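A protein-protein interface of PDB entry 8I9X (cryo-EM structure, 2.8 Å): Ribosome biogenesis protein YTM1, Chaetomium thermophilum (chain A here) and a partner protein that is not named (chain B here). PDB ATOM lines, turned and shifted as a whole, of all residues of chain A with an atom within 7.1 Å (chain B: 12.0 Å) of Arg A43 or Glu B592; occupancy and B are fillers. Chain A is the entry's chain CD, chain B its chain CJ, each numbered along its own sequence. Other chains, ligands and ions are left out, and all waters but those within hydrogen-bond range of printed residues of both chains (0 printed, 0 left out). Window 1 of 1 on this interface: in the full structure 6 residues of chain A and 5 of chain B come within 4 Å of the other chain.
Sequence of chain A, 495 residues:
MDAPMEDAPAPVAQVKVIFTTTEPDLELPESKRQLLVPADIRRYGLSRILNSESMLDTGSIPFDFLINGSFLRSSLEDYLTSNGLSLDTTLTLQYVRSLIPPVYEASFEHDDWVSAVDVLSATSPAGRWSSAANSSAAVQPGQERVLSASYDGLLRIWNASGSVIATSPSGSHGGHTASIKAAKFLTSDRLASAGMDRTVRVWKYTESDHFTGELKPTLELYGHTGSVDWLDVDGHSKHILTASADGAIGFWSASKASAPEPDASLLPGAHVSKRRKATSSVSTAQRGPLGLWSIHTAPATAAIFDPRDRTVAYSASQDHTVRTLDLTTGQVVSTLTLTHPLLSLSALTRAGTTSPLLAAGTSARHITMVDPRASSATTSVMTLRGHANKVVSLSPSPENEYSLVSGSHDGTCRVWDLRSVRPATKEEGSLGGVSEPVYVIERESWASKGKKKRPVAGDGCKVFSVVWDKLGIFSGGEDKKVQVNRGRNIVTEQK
The guanidinium group of Arg B589 is in hydrogen-bond range of the backbone carbonyl oxygen of Leu B585 (2.7 Å).
Of chain A, only Arg A43 and Tyr A44 come within 4 Å of Glu B592.
Of chain B, only Glu B592 (2.7 Å) comes within 4 Å of Tyr A44.
No residue of chain B comes within 4 Å of Gly A45.
No residue of chain B comes within 4 Å of Pro A62.
No residue of chain B comes within 4 Å of Phe A65.
No residue of chain B comes within 4 Å of Leu A72.
Printed residues of chain B within 4 Å of Arg A73: Arg B589.
Of the printed residues of chain A, Arg B589 touches Arg A73 (3.2 Å).
Of the printed residues of chain A, Gln B588 touches Arg A42.
Asp A64 touches none of the printed residues of chain B.
Thr B584 touches none of the printed residues of chain A.
The nearest printed residue of chain B that does not touch Arg A73 is Leu B585 (5.1 Å).
Of the 13 printed residues of chain B, 3 touch a printed residue of chain A.
Of the 17 printed residues of chain A, 4 touch a printed residue of chain B.
Hydrophobic or aromatic side chains of chain A that line the printed part of chain B: Tyr A44.
Among the printed residues, Asp or Glu carboxylates within 4 Å of a Lys or Arg side-chain nitrogen of the other chain: Arg A43 with Glu B592.
Among the printed residues, merely in contact across the chains: Arg A42 with Gln B588 (3.7 Å).
The side-chain carboxylate (OE2) of Glu B592 is in hydrogen-bond range of the backbone NH (N) of Tyr A44.
NH2 of Arg A73 sits close to NH1 of Arg B589 (3.2 Å).
The side-chain carboxylate (OE1) of Glu B592 lies within salt-bridge range of the guanidinium group (NH2) of Arg A43, at 3.5 Å.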
ATOM      1  N   ILE A  41       1.929  -9.155  -4.362  1.00  0.00           N
ATOM      2  CA  ILE A  41       1.061  -8.145  -3.772  1.00  0.00           C
ATOM      3  C   ILE A  41       1.137  -6.851  -4.580  1.00  0.00           C
ATOM      4  O   ILE A  41       2.161  -6.514  -5.181  1.00  0.00           O
ATOM      5  CB  ILE A  41       1.430  -7.915  -2.292  1.00  0.00           C
ATOM      6  CG1 ILE A  41       1.298  -9.222  -1.513  1.00  0.00           C
ATOM      7  CG2 ILE A  41       0.536  -6.866  -1.648  1.00  0.00           C
ATOM      8  CD1 ILE A  41      -0.104  -9.795  -1.513  1.00  0.00           C
ATOM      9  N   ARG A  42       0.027  -6.120  -4.590  1.00  0.00           N
ATOM     10  CA  ARG A  42      -0.095  -4.827  -5.241  1.00  0.00           C
ATOM     11  C   ARG A  42       0.447  -3.722  -4.345  1.00  0.00           C
ATOM     12  O   ARG A  42       0.650  -3.905  -3.139  1.00  0.00           O
ATOM     13  CB  ARG A  42      -1.561  -4.528  -5.586  1.00  0.00           C
ATOM     14  CG  ARG A  42      -2.203  -5.461  -6.604  1.00  0.00           C
ATOM     15  CD  ARG A  42      -1.566  -5.322  -7.980  1.00  0.00           C
ATOM     16  NE  ARG A  42      -0.382  -6.148  -8.167  1.00  0.00           N
ATOM     17  CZ  ARG A  42       0.467  -6.009  -9.176  1.00  0.00           C
ATOM     18  NH1 ARG A  42       0.294  -5.080 -10.102  1.00  0.00           N
ATOM     19  NH2 ARG A  42       1.515  -6.821  -9.258  1.00  0.00           N
ATOM     20  N   ARG A  43       0.674  -2.558  -4.960  1.00  0.00           N
ATOM     21  CA  ARG A  43       1.035  -1.382  -4.181  1.00  0.00           C
ATOM     22  C   ARG A  43      -0.067  -1.025  -3.199  1.00  0.00           C
ATOM     23  O   ARG A  43       0.218  -0.573  -2.088  1.00  0.00           O
ATOM     24  CB  ARG A  43       1.334  -0.197  -5.101  1.00  0.00           C
ATOM     25  CG  ARG A  43       2.085   0.934  -4.411  1.00  0.00           C
ATOM     26  CD  ARG A  43       1.155   2.039  -3.930  1.00  0.00           C
ATOM     27  NE  ARG A  43       0.451   2.686  -5.030  1.00  0.00           N
ATOM     28  CZ  ARG A  43      -0.582   3.504  -4.879  1.00  0.00           C
ATOM     29  NH1 ARG A  43      -1.067   3.791  -3.682  1.00  0.00           N
ATOM     30  NH2 ARG A  43      -1.139   4.051  -5.956  1.00  0.00           N
ATOM     31  N   TYR A  44      -1.327  -1.230  -3.588  1.00  0.00           N
ATOM     32  CA  TYR A  44      -2.441  -1.046  -2.664  1.00  0.00           C
ATOM     33  C   TYR A  44      -2.288  -1.943  -1.442  1.00  0.00           C
ATOM     34  O   TYR A  44      -2.419  -1.487  -0.298  1.00  0.00           O
ATOM     35  CB  TYR A  44      -3.755  -1.341  -3.387  1.00  0.00           C
ATOM     36  CG  TYR A  44      -4.996  -0.873  -2.665  1.00  0.00           C
ATOM     37  CD1 TYR A  44      -5.211   0.475  -2.412  1.00  0.00           C
ATOM     38  CD2 TYR A  44      -5.957  -1.782  -2.242  1.00  0.00           C
ATOM     39  CE1 TYR A  44      -6.349   0.904  -1.758  1.00  0.00           C
ATOM     40  CE2 TYR A  44      -7.096  -1.362  -1.585  1.00  0.00           C
ATOM     41  CZ  TYR A  44      -7.287  -0.019  -1.344  1.00  0.00           C
ATOM     42  OH  TYR A  44      -8.421   0.404  -0.689  1.00  0.00           O
ATOM     43  N   GLY A  45      -1.998  -3.227  -1.668  1.00  0.00           N
ATOM     44  CA  GLY A  45      -1.847  -4.154  -0.561  1.00  0.00           C
ATOM     45  C   GLY A  45      -0.685  -3.833   0.349  1.00  0.00           C
ATOM     46  O   GLY A  45      -0.826  -3.876   1.575  1.00  0.00           O
ATOM     47  N   LEU A  46       0.472  -3.491  -0.220  1.00  0.00           N
ATOM     48  CA  LEU A  46       1.603  -3.152   0.633  1.00  0.00           C
ATOM     49  C   LEU A  46       1.441  -1.792   1.305  1.00  0.00           C
ATOM     50  O   LEU A  46       1.968  -1.596   2.404  1.00  0.00           O
ATOM     51  CB  LEU A  46       2.908  -3.223  -0.166  1.00  0.00           C
ATOM     52  CG  LEU A  46       3.097  -2.374  -1.423  1.00  0.00           C
ATOM     53  CD1 LEU A  46       3.721  -1.037  -1.091  1.00  0.00           C
ATOM     54  CD2 LEU A  46       3.936  -3.127  -2.445  1.00  0.00           C
ATOM     55  N   SER A  47       0.694  -0.866   0.699  1.00  0.00           N
ATOM     56  CA  SER A  47       0.361   0.380   1.378  1.00  0.00           C
ATOM     57  C   SER A  47      -0.550   0.118   2.570  1.00  0.00           C
ATOM     58  O   SER A  47      -0.373   0.708   3.641  1.00  0.00           O
ATOM     59  CB  SER A  47      -0.296   1.353   0.400  1.00  0.00           C
ATOM     60  OG  SER A  47      -0.792   2.497   1.072  1.00  0.00           O
ATOM     61  N   ARG A  48      -1.530  -0.772   2.404  1.00  0.00           N
ATOM     62  CA  ARG A  48      -2.330  -1.200   3.545  1.00  0.00           C
ATOM     63  C   ARG A  48      -1.478  -1.869   4.616  1.00  0.00           C
ATOM     64  O   ARG A  48      -1.708  -1.641   5.809  1.00  0.00           O
ATOM     65  CB  ARG A  48      -3.439  -2.152   3.093  1.00  0.00           C
ATOM     66  CG  ARG A  48      -4.468  -1.555   2.133  1.00  0.00           C
ATOM     67  CD  ARG A  48      -5.464  -0.631   2.833  1.00  0.00           C
ATOM     68  NE  ARG A  48      -4.903   0.671   3.174  1.00  0.00           N
ATOM     69  CZ  ARG A  48      -4.726   1.661   2.310  1.00  0.00           C
ATOM     70  NH1 ARG A  48      -5.053   1.532   1.035  1.00  0.00           N
ATOM     71  NH2 ARG A  48      -4.211   2.810   2.736  1.00  0.00           N
ATOM     72  N   ILE A  49      -0.502  -2.684   4.213  1.00  0.00           N
ATOM     73  CA  ILE A  49       0.394  -3.318   5.181  1.00  0.00           C
ATOM     74  C   ILE A  49       1.159  -2.260   5.968  1.00  0.00           C
ATOM     75  O   ILE A  49       1.258  -2.326   7.199  1.00  0.00           O
ATOM     76  CB  ILE A  49       1.352  -4.290   4.471  1.00  0.00           C
ATOM     77  CG1 ILE A  49       0.630  -5.588   4.110  1.00  0.00           C
ATOM     78  CG2 ILE A  49       2.570  -4.576   5.339  1.00  0.00           C
ATOM     79  CD1 ILE A  49       1.520  -6.605   3.430  1.00  0.00           C
ATOM     80  N   PRO A  62      -1.241   8.168   1.909  1.00  0.00           N
ATOM     81  CA  PRO A  62      -0.558   7.482   0.803  1.00  0.00           C
ATOM     82  C   PRO A  62       0.956   7.572   0.890  1.00  0.00           C
ATOM     83  O   PRO A  62       1.503   8.547   1.413  1.00  0.00           O
ATOM     84  CB  PRO A  62      -1.084   8.212  -0.440  1.00  0.00           C
ATOM     85  CG  PRO A  62      -2.350   8.870   0.000  1.00  0.00           C
ATOM     86  CD  PRO A  62      -2.114   9.251   1.429  1.00  0.00           C
ATOM     87  N   PHE A  63       1.640   6.555   0.369  1.00  0.00           N
ATOM     88  CA  PHE A  63       3.088   6.564   0.223  1.00  0.00           C
ATOM     89  C   PHE A  63       3.469   5.973  -1.125  1.00  0.00           C
ATOM     90  O   PHE A  63       2.803   5.065  -1.629  1.00  0.00           O
ATOM     91  CB  PHE A  63       3.793   5.780   1.338  1.00  0.00           C
ATOM     92  CG  PHE A  63       3.194   5.976   2.699  1.00  0.00           C
ATOM     93  CD1 PHE A  63       3.403   7.154   3.397  1.00  0.00           C
ATOM     94  CD2 PHE A  63       2.439   4.980   3.288  1.00  0.00           C
ATOM     95  CE1 PHE A  63       2.860   7.337   4.652  1.00  0.00           C
ATOM     96  CE2 PHE A  63       1.901   5.155   4.544  1.00  0.00           C
ATOM     97  CZ  PHE A  63       2.108   6.336   5.225  1.00  0.00           C
ATOM     98  N   ASP A  64       4.525   6.520  -1.715  1.00  0.00           N
ATOM     99  CA  ASP A  64       5.152   5.965  -2.901  1.00  0.00           C
ATOM    100  C   ASP A  64       6.451   5.276  -2.501  1.00  0.00           C
ATOM    101  O   ASP A  64       7.021   5.558  -1.443  1.00  0.00           O
ATOM    102  CB  ASP A  64       5.382   7.050  -3.971  1.00  0.00           C
ATOM    103  CG  ASP A  64       6.328   8.150  -3.514  1.00  0.00           C
ATOM    104  OD1 ASP A  64       6.789   8.122  -2.357  1.00  0.00           O
ATOM    105  OD2 ASP A  64       6.603   9.062  -4.322  1.00  0.00           O
ATOM    106  N   PHE A  65       6.901   4.345  -3.337  1.00  0.00           N
ATOM    107  CA  PHE A  65       7.943   3.407  -2.950  1.00  0.00           C
ATOM    108  C   PHE A  65       8.987   3.301  -4.053  1.00  0.00           C
ATOM    109  O   PHE A  65       8.647   3.181  -5.233  1.00  0.00           O
ATOM    110  CB  PHE A  65       7.329   2.039  -2.649  1.00  0.00           C
ATOM    111  CG  PHE A  65       6.232   2.090  -1.619  1.00  0.00           C
ATOM    112  CD1 PHE A  65       6.510   1.939  -0.274  1.00  0.00           C
ATOM    113  CD2 PHE A  65       4.917   2.298  -2.003  1.00  0.00           C
ATOM    114  CE1 PHE A  65       5.502   1.990   0.671  1.00  0.00           C
ATOM    115  CE2 PHE A  65       3.905   2.352  -1.064  1.00  0.00           C
ATOM    116  CZ  PHE A  65       4.198   2.198   0.274  1.00  0.00           C
ATOM    117  N   LEU A  72       8.307   1.554  -7.706  1.00  0.00           N
ATOM    118  CA  LEU A  72       7.755   0.205  -7.814  1.00  0.00           C
ATOM    119  C   LEU A  72       6.511   0.275  -8.693  1.00  0.00           C
ATOM    120  O   LEU A  72       5.449   0.722  -8.253  1.00  0.00           O
ATOM    121  CB  LEU A  72       7.438  -0.367  -6.436  1.00  0.00           C
ATOM    122  CG  LEU A  72       6.993  -1.831  -6.396  1.00  0.00           C
ATOM    123  CD1 LEU A  72       8.174  -2.764  -6.625  1.00  0.00           C
ATOM    124  CD2 LEU A  72       6.308  -2.146  -5.075  1.00  0.00           C
ATOM    125  N   ARG A  73       6.647  -0.174  -9.941  1.00  0.00           N
ATOM    126  CA  ARG A  73       5.558  -0.125 -10.904  1.00  0.00           C
ATOM    127  C   ARG A  73       4.847  -1.455 -11.098  1.00  0.00           C
ATOM    128  O   ARG A  73       3.682  -1.457 -11.504  1.00  0.00           O
ATOM    129  CB  ARG A  73       6.072   0.361 -12.267  1.00  0.00           C
ATOM    130  CG  ARG A  73       6.588   1.796 -12.282  1.00  0.00           C
ATOM    131  CD  ARG A  73       5.719   2.770 -11.488  1.00  0.00           C
ATOM    132  NE  ARG A  73       4.330   2.768 -11.933  1.00  0.00           N
ATOM    133  CZ  ARG A  73       3.298   2.386 -11.191  1.00  0.00           C
ATOM    134  NH1 ARG A  73       3.449   2.036  -9.924  1.00  0.00           N
ATOM    135  NH2 ARG A  73       2.084   2.370 -11.730  1.00  0.00           N
ATOM    136  N   SER A  74       5.507  -2.572 -10.821  1.00  0.00           N
ATOM    137  CA  SER A  74       4.944  -3.897 -11.030  1.00  0.00           C
ATOM    138  C   SER A  74       5.058  -4.711  -9.741  1.00  0.00           C
ATOM    139  O   SER A  74       5.389  -4.186  -8.675  1.00  0.00           O
ATOM    140  CB  SER A  74       5.643  -4.591 -12.199  1.00  0.00           C
ATOM    141  OG  SER A  74       7.009  -4.826 -11.905  1.00  0.00           O
ATOM    142  N   SER A  98       3.304  10.388  -0.788  1.00  0.00           N
ATOM    143  CA  SER A  98       2.784  10.521  -2.140  1.00  0.00           C
ATOM    144  C   SER A  98       2.300  11.941  -2.404  1.00  0.00           C
ATOM    145  O   SER A  98       1.701  12.586  -1.537  1.00  0.00           O
ATOM    146  CB  SER A  98       1.634   9.545  -2.380  1.00  0.00           C
ATOM    147  OG  SER A  98       2.088   8.207  -2.369  1.00  0.00           O
ATOM    148  N   GLU B 582      -2.325   0.454 -20.588  1.00  0.00           N
ATOM    149  CA  GLU B 582      -2.361   1.880 -20.284  1.00  0.00           C
ATOM    150  C   GLU B 582      -3.580   2.227 -19.435  1.00  0.00           C
ATOM    151  O   GLU B 582      -3.445   2.638 -18.281  1.00  0.00           O
ATOM    152  CB  GLU B 582      -2.363   2.704 -21.574  1.00  0.00           C
ATOM    153  CG  GLU B 582      -0.988   2.887 -22.199  1.00  0.00           C
ATOM    154  CD  GLU B 582      -0.107   3.823 -21.395  1.00  0.00           C
ATOM    155  OE1 GLU B 582      -0.651   4.754 -20.765  1.00  0.00           O
ATOM    156  OE2 GLU B 582       1.128   3.632 -21.397  1.00  0.00           O
ATOM    157  N   ALA B 583      -4.769   2.022 -20.001  1.00  0.00           N
ATOM    158  CA  ALA B 583      -6.012   2.338 -19.309  1.00  0.00           C
ATOM    159  C   ALA B 583      -6.015   1.718 -17.918  1.00  0.00           C
ATOM    160  O   ALA B 583      -6.315   2.399 -16.931  1.00  0.00           O
ATOM    161  CB  ALA B 583      -7.215   1.844 -20.115  1.00  0.00           C
ATOM    162  N   THR B 584      -5.637   0.440 -17.834  1.00  0.00           N
ATOM    163  CA  THR B 584      -5.525  -0.223 -16.540  1.00  0.00           C
ATOM    164  C   THR B 584      -4.505   0.475 -15.648  1.00  0.00           C
ATOM    165  O   THR B 584      -4.700   0.571 -14.438  1.00  0.00           O
ATOM    166  CB  THR B 584      -5.149  -1.694 -16.729  1.00  0.00           C
ATOM    167  OG1 THR B 584      -4.098  -1.804 -17.697  1.00  0.00           O
ATOM    168  CG2 THR B 584      -6.354  -2.503 -17.188  1.00  0.00           C
ATOM    169  N   LEU B 585      -3.429   0.990 -16.235  1.00  0.00           N
ATOM    170  CA  LEU B 585      -2.330   1.642 -15.526  1.00  0.00           C
ATOM    171  C   LEU B 585      -2.759   2.946 -14.834  1.00  0.00           C
ATOM    172  O   LEU B 585      -2.664   3.075 -13.594  1.00  0.00           O
ATOM    173  CB  LEU B 585      -1.193   1.807 -16.555  1.00  0.00           C
ATOM    174  CG  LEU B 585       0.242   2.323 -16.529  1.00  0.00           C
ATOM    175  CD1 LEU B 585       1.066   1.558 -17.537  1.00  0.00           C
ATOM    176  CD2 LEU B 585       0.239   3.769 -16.951  1.00  0.00           C
ATOM    177  N   GLU B 586      -3.262   3.913 -15.609  1.00  0.00           N
ATOM    178  CA  GLU B 586      -3.754   5.124 -14.954  1.00  0.00           C
ATOM    179  C   GLU B 586      -4.981   4.866 -14.080  1.00  0.00           C
ATOM    180  O   GLU B 586      -5.104   5.467 -13.005  1.00  0.00           O
ATOM    181  CB  GLU B 586      -4.054   6.254 -15.955  1.00  0.00           C
ATOM    182  CG  GLU B 586      -2.838   6.860 -16.669  1.00  0.00           C
ATOM    183  CD  GLU B 586      -2.376   6.082 -17.873  1.00  0.00           C
ATOM    184  OE1 GLU B 586      -3.034   5.091 -18.217  1.00  0.00           O
ATOM    185  OE2 GLU B 586      -1.352   6.464 -18.478  1.00  0.00           O
ATOM    186  N   ARG B 587      -5.898   3.988 -14.504  1.00  0.00           N
ATOM    187  CA  ARG B 587      -7.031   3.665 -13.648  1.00  0.00           C
ATOM    188  C   ARG B 587      -6.573   3.019 -12.349  1.00  0.00           C
ATOM    189  O   ARG B 587      -7.213   3.196 -11.307  1.00  0.00           O
ATOM    190  CB  ARG B 587      -8.007   2.752 -14.391  1.00  0.00           C
ATOM    191  CG  ARG B 587      -9.270   2.422 -13.613  1.00  0.00           C
ATOM    192  CD  ARG B 587     -10.216   1.552 -14.429  1.00  0.00           C
ATOM    193  NE  ARG B 587      -9.604   0.289 -14.826  1.00  0.00           N
ATOM    194  CZ  ARG B 587     -10.095  -0.523 -15.753  1.00  0.00           C
ATOM    195  NH1 ARG B 587     -11.209  -0.235 -16.406  1.00  0.00           N
ATOM    196  NH2 ARG B 587      -9.452  -1.655 -16.030  1.00  0.00           N
ATOM    197  N   GLN B 588      -5.464   2.282 -12.385  1.00  0.00           N
ATOM    198  CA  GLN B 588      -4.920   1.638 -11.203  1.00  0.00           C
ATOM    199  C   GLN B 588      -4.429   2.679 -10.212  1.00  0.00           C
ATOM    200  O   GLN B 588      -4.790   2.608  -9.033  1.00  0.00           O
ATOM    201  CB  GLN B 588      -3.795   0.673 -11.580  1.00  0.00           C
ATOM    202  CG  GLN B 588      -3.448  -0.312 -10.476  1.00  0.00           C
ATOM    203  CD  GLN B 588      -2.389  -1.312 -10.894  1.00  0.00           C
ATOM    204  OE1 GLN B 588      -1.860  -1.247 -12.004  1.00  0.00           O
ATOM    205  NE2 GLN B 588      -2.077  -2.248 -10.006  1.00  0.00           N
ATOM    206  N   ARG B 589      -3.624   3.655 -10.653  1.00  0.00           N
ATOM    207  CA  ARG B 589      -3.295   4.710  -9.687  1.00  0.00           C
ATOM    208  C   ARG B 589      -4.531   5.462  -9.210  1.00  0.00           C
ATOM    209  O   ARG B 589      -4.628   5.805  -8.030  1.00  0.00           O
ATOM    210  CB  ARG B 589      -2.245   5.721 -10.158  1.00  0.00           C
ATOM    211  CG  ARG B 589      -0.805   5.266 -10.044  1.00  0.00           C
ATOM    212  CD  ARG B 589      -0.346   4.434 -11.159  1.00  0.00           C
ATOM    213  NE  ARG B 589      -0.358   5.274 -12.344  1.00  0.00           N
ATOM    214  CZ  ARG B 589      -0.240   4.813 -13.573  1.00  0.00           C
ATOM    215  NH1 ARG B 589      -0.012   3.534 -13.799  1.00  0.00           N
ATOM    216  NH2 ARG B 589      -0.338   5.659 -14.594  1.00  0.00           N
ATOM    217  N   GLU B 590      -5.476   5.754 -10.105  1.00  0.00           N
ATOM    218  CA  GLU B 590      -6.651   6.512  -9.676  1.00  0.00           C
ATOM    219  C   GLU B 590      -7.402   5.778  -8.567  1.00  0.00           C
ATOM    220  O   GLU B 590      -7.697   6.350  -7.507  1.00  0.00           O
ATOM    221  CB  GLU B 590      -7.569   6.777 -10.869  1.00  0.00           C
ATOM    222  CG  GLU B 590      -8.725   7.721 -10.569  1.00  0.00           C
ATOM    223  CD  GLU B 590      -9.971   6.997 -10.100  1.00  0.00           C
ATOM    224  OE1 GLU B 590     -10.188   5.845 -10.531  1.00  0.00           O
ATOM    225  OE2 GLU B 590     -10.734   7.580  -9.302  1.00  0.00           O
ATOM    226  N   LEU B 591      -7.693   4.495  -8.786  1.00  0.00           N
ATOM    227  CA  LEU B 591      -8.439   3.712  -7.808  1.00  0.00           C
ATOM    228  C   LEU B 591      -7.641   3.525  -6.524  1.00  0.00           C
ATOM    229  O   LEU B 591      -8.197   3.600  -5.421  1.00  0.00           O
ATOM    230  CB  LEU B 591      -8.827   2.362  -8.409  1.00  0.00           C
ATOM    231  CG  LEU B 591     -10.075   2.367  -9.296  1.00  0.00           C
ATOM    232  CD1 LEU B 591     -10.151   1.095 -10.125  1.00  0.00           C
ATOM    233  CD2 LEU B 591     -11.336   2.542  -8.460  1.00  0.00           C
ATOM    234  N   GLU B 592      -6.333   3.275  -6.640  1.00  0.00           N
ATOM    235  CA  GLU B 592      -5.511   3.076  -5.452  1.00  0.00           C
ATOM    236  C   GLU B 592      -5.436   4.346  -4.615  1.00  0.00           C
ATOM    237  O   GLU B 592      -5.506   4.298  -3.381  1.00  0.00           O
ATOM    238  CB  GLU B 592      -4.116   2.608  -5.862  1.00  0.00           C
ATOM    239  CG  GLU B 592      -4.001   1.104  -6.038  1.00  0.00           C
ATOM    240  CD  GLU B 592      -2.676   0.684  -6.639  1.00  0.00           C
ATOM    241  OE1 GLU B 592      -2.319   1.205  -7.717  1.00  0.00           O
ATOM    242  OE2 GLU B 592      -1.990  -0.169  -6.036  1.00  0.00           O
ATOM    243  N   ALA B 593      -5.289   5.499  -5.274  1.00  0.00           N
ATOM    244  CA  ALA B 593      -5.281   6.780  -4.583  1.00  0.00           C
ATOM    245  C   ALA B 593      -6.606   7.019  -3.875  1.00  0.00           C
ATOM    246  O   ALA B 593      -6.639   7.465  -2.721  1.00  0.00           O
ATOM    247  CB  ALA B 593      -4.985   7.906  -5.579  1.00  0.00           C
ATOM    248  N   GLU B 594      -7.711   6.721  -4.550  1.00  0.00           N
ATOM    249  CA  GLU B 594      -9.006   6.801  -3.890  1.00  0.00           C
ATOM    250  C   GLU B 594      -9.270   5.531  -3.088  1.00  0.00           C
ATOM    251  O   GLU B 594      -8.419   5.087  -2.316  1.00  0.00           O
ATOM    252  CB  GLU B 594     -10.127   7.035  -4.902  1.00  0.00           C
ATOM    253  CG  GLU B 594     -11.517   7.018  -4.285  1.00  0.00           C
ATOM    254  CD  GLU B 594     -11.727   8.131  -3.274  1.00  0.00           C
ATOM    255  OE1 GLU B 594     -11.086   9.195  -3.411  1.00  0.00           O
ATOM    256  OE2 GLU B 594     -12.533   7.939  -2.339  1.00  0.00           O
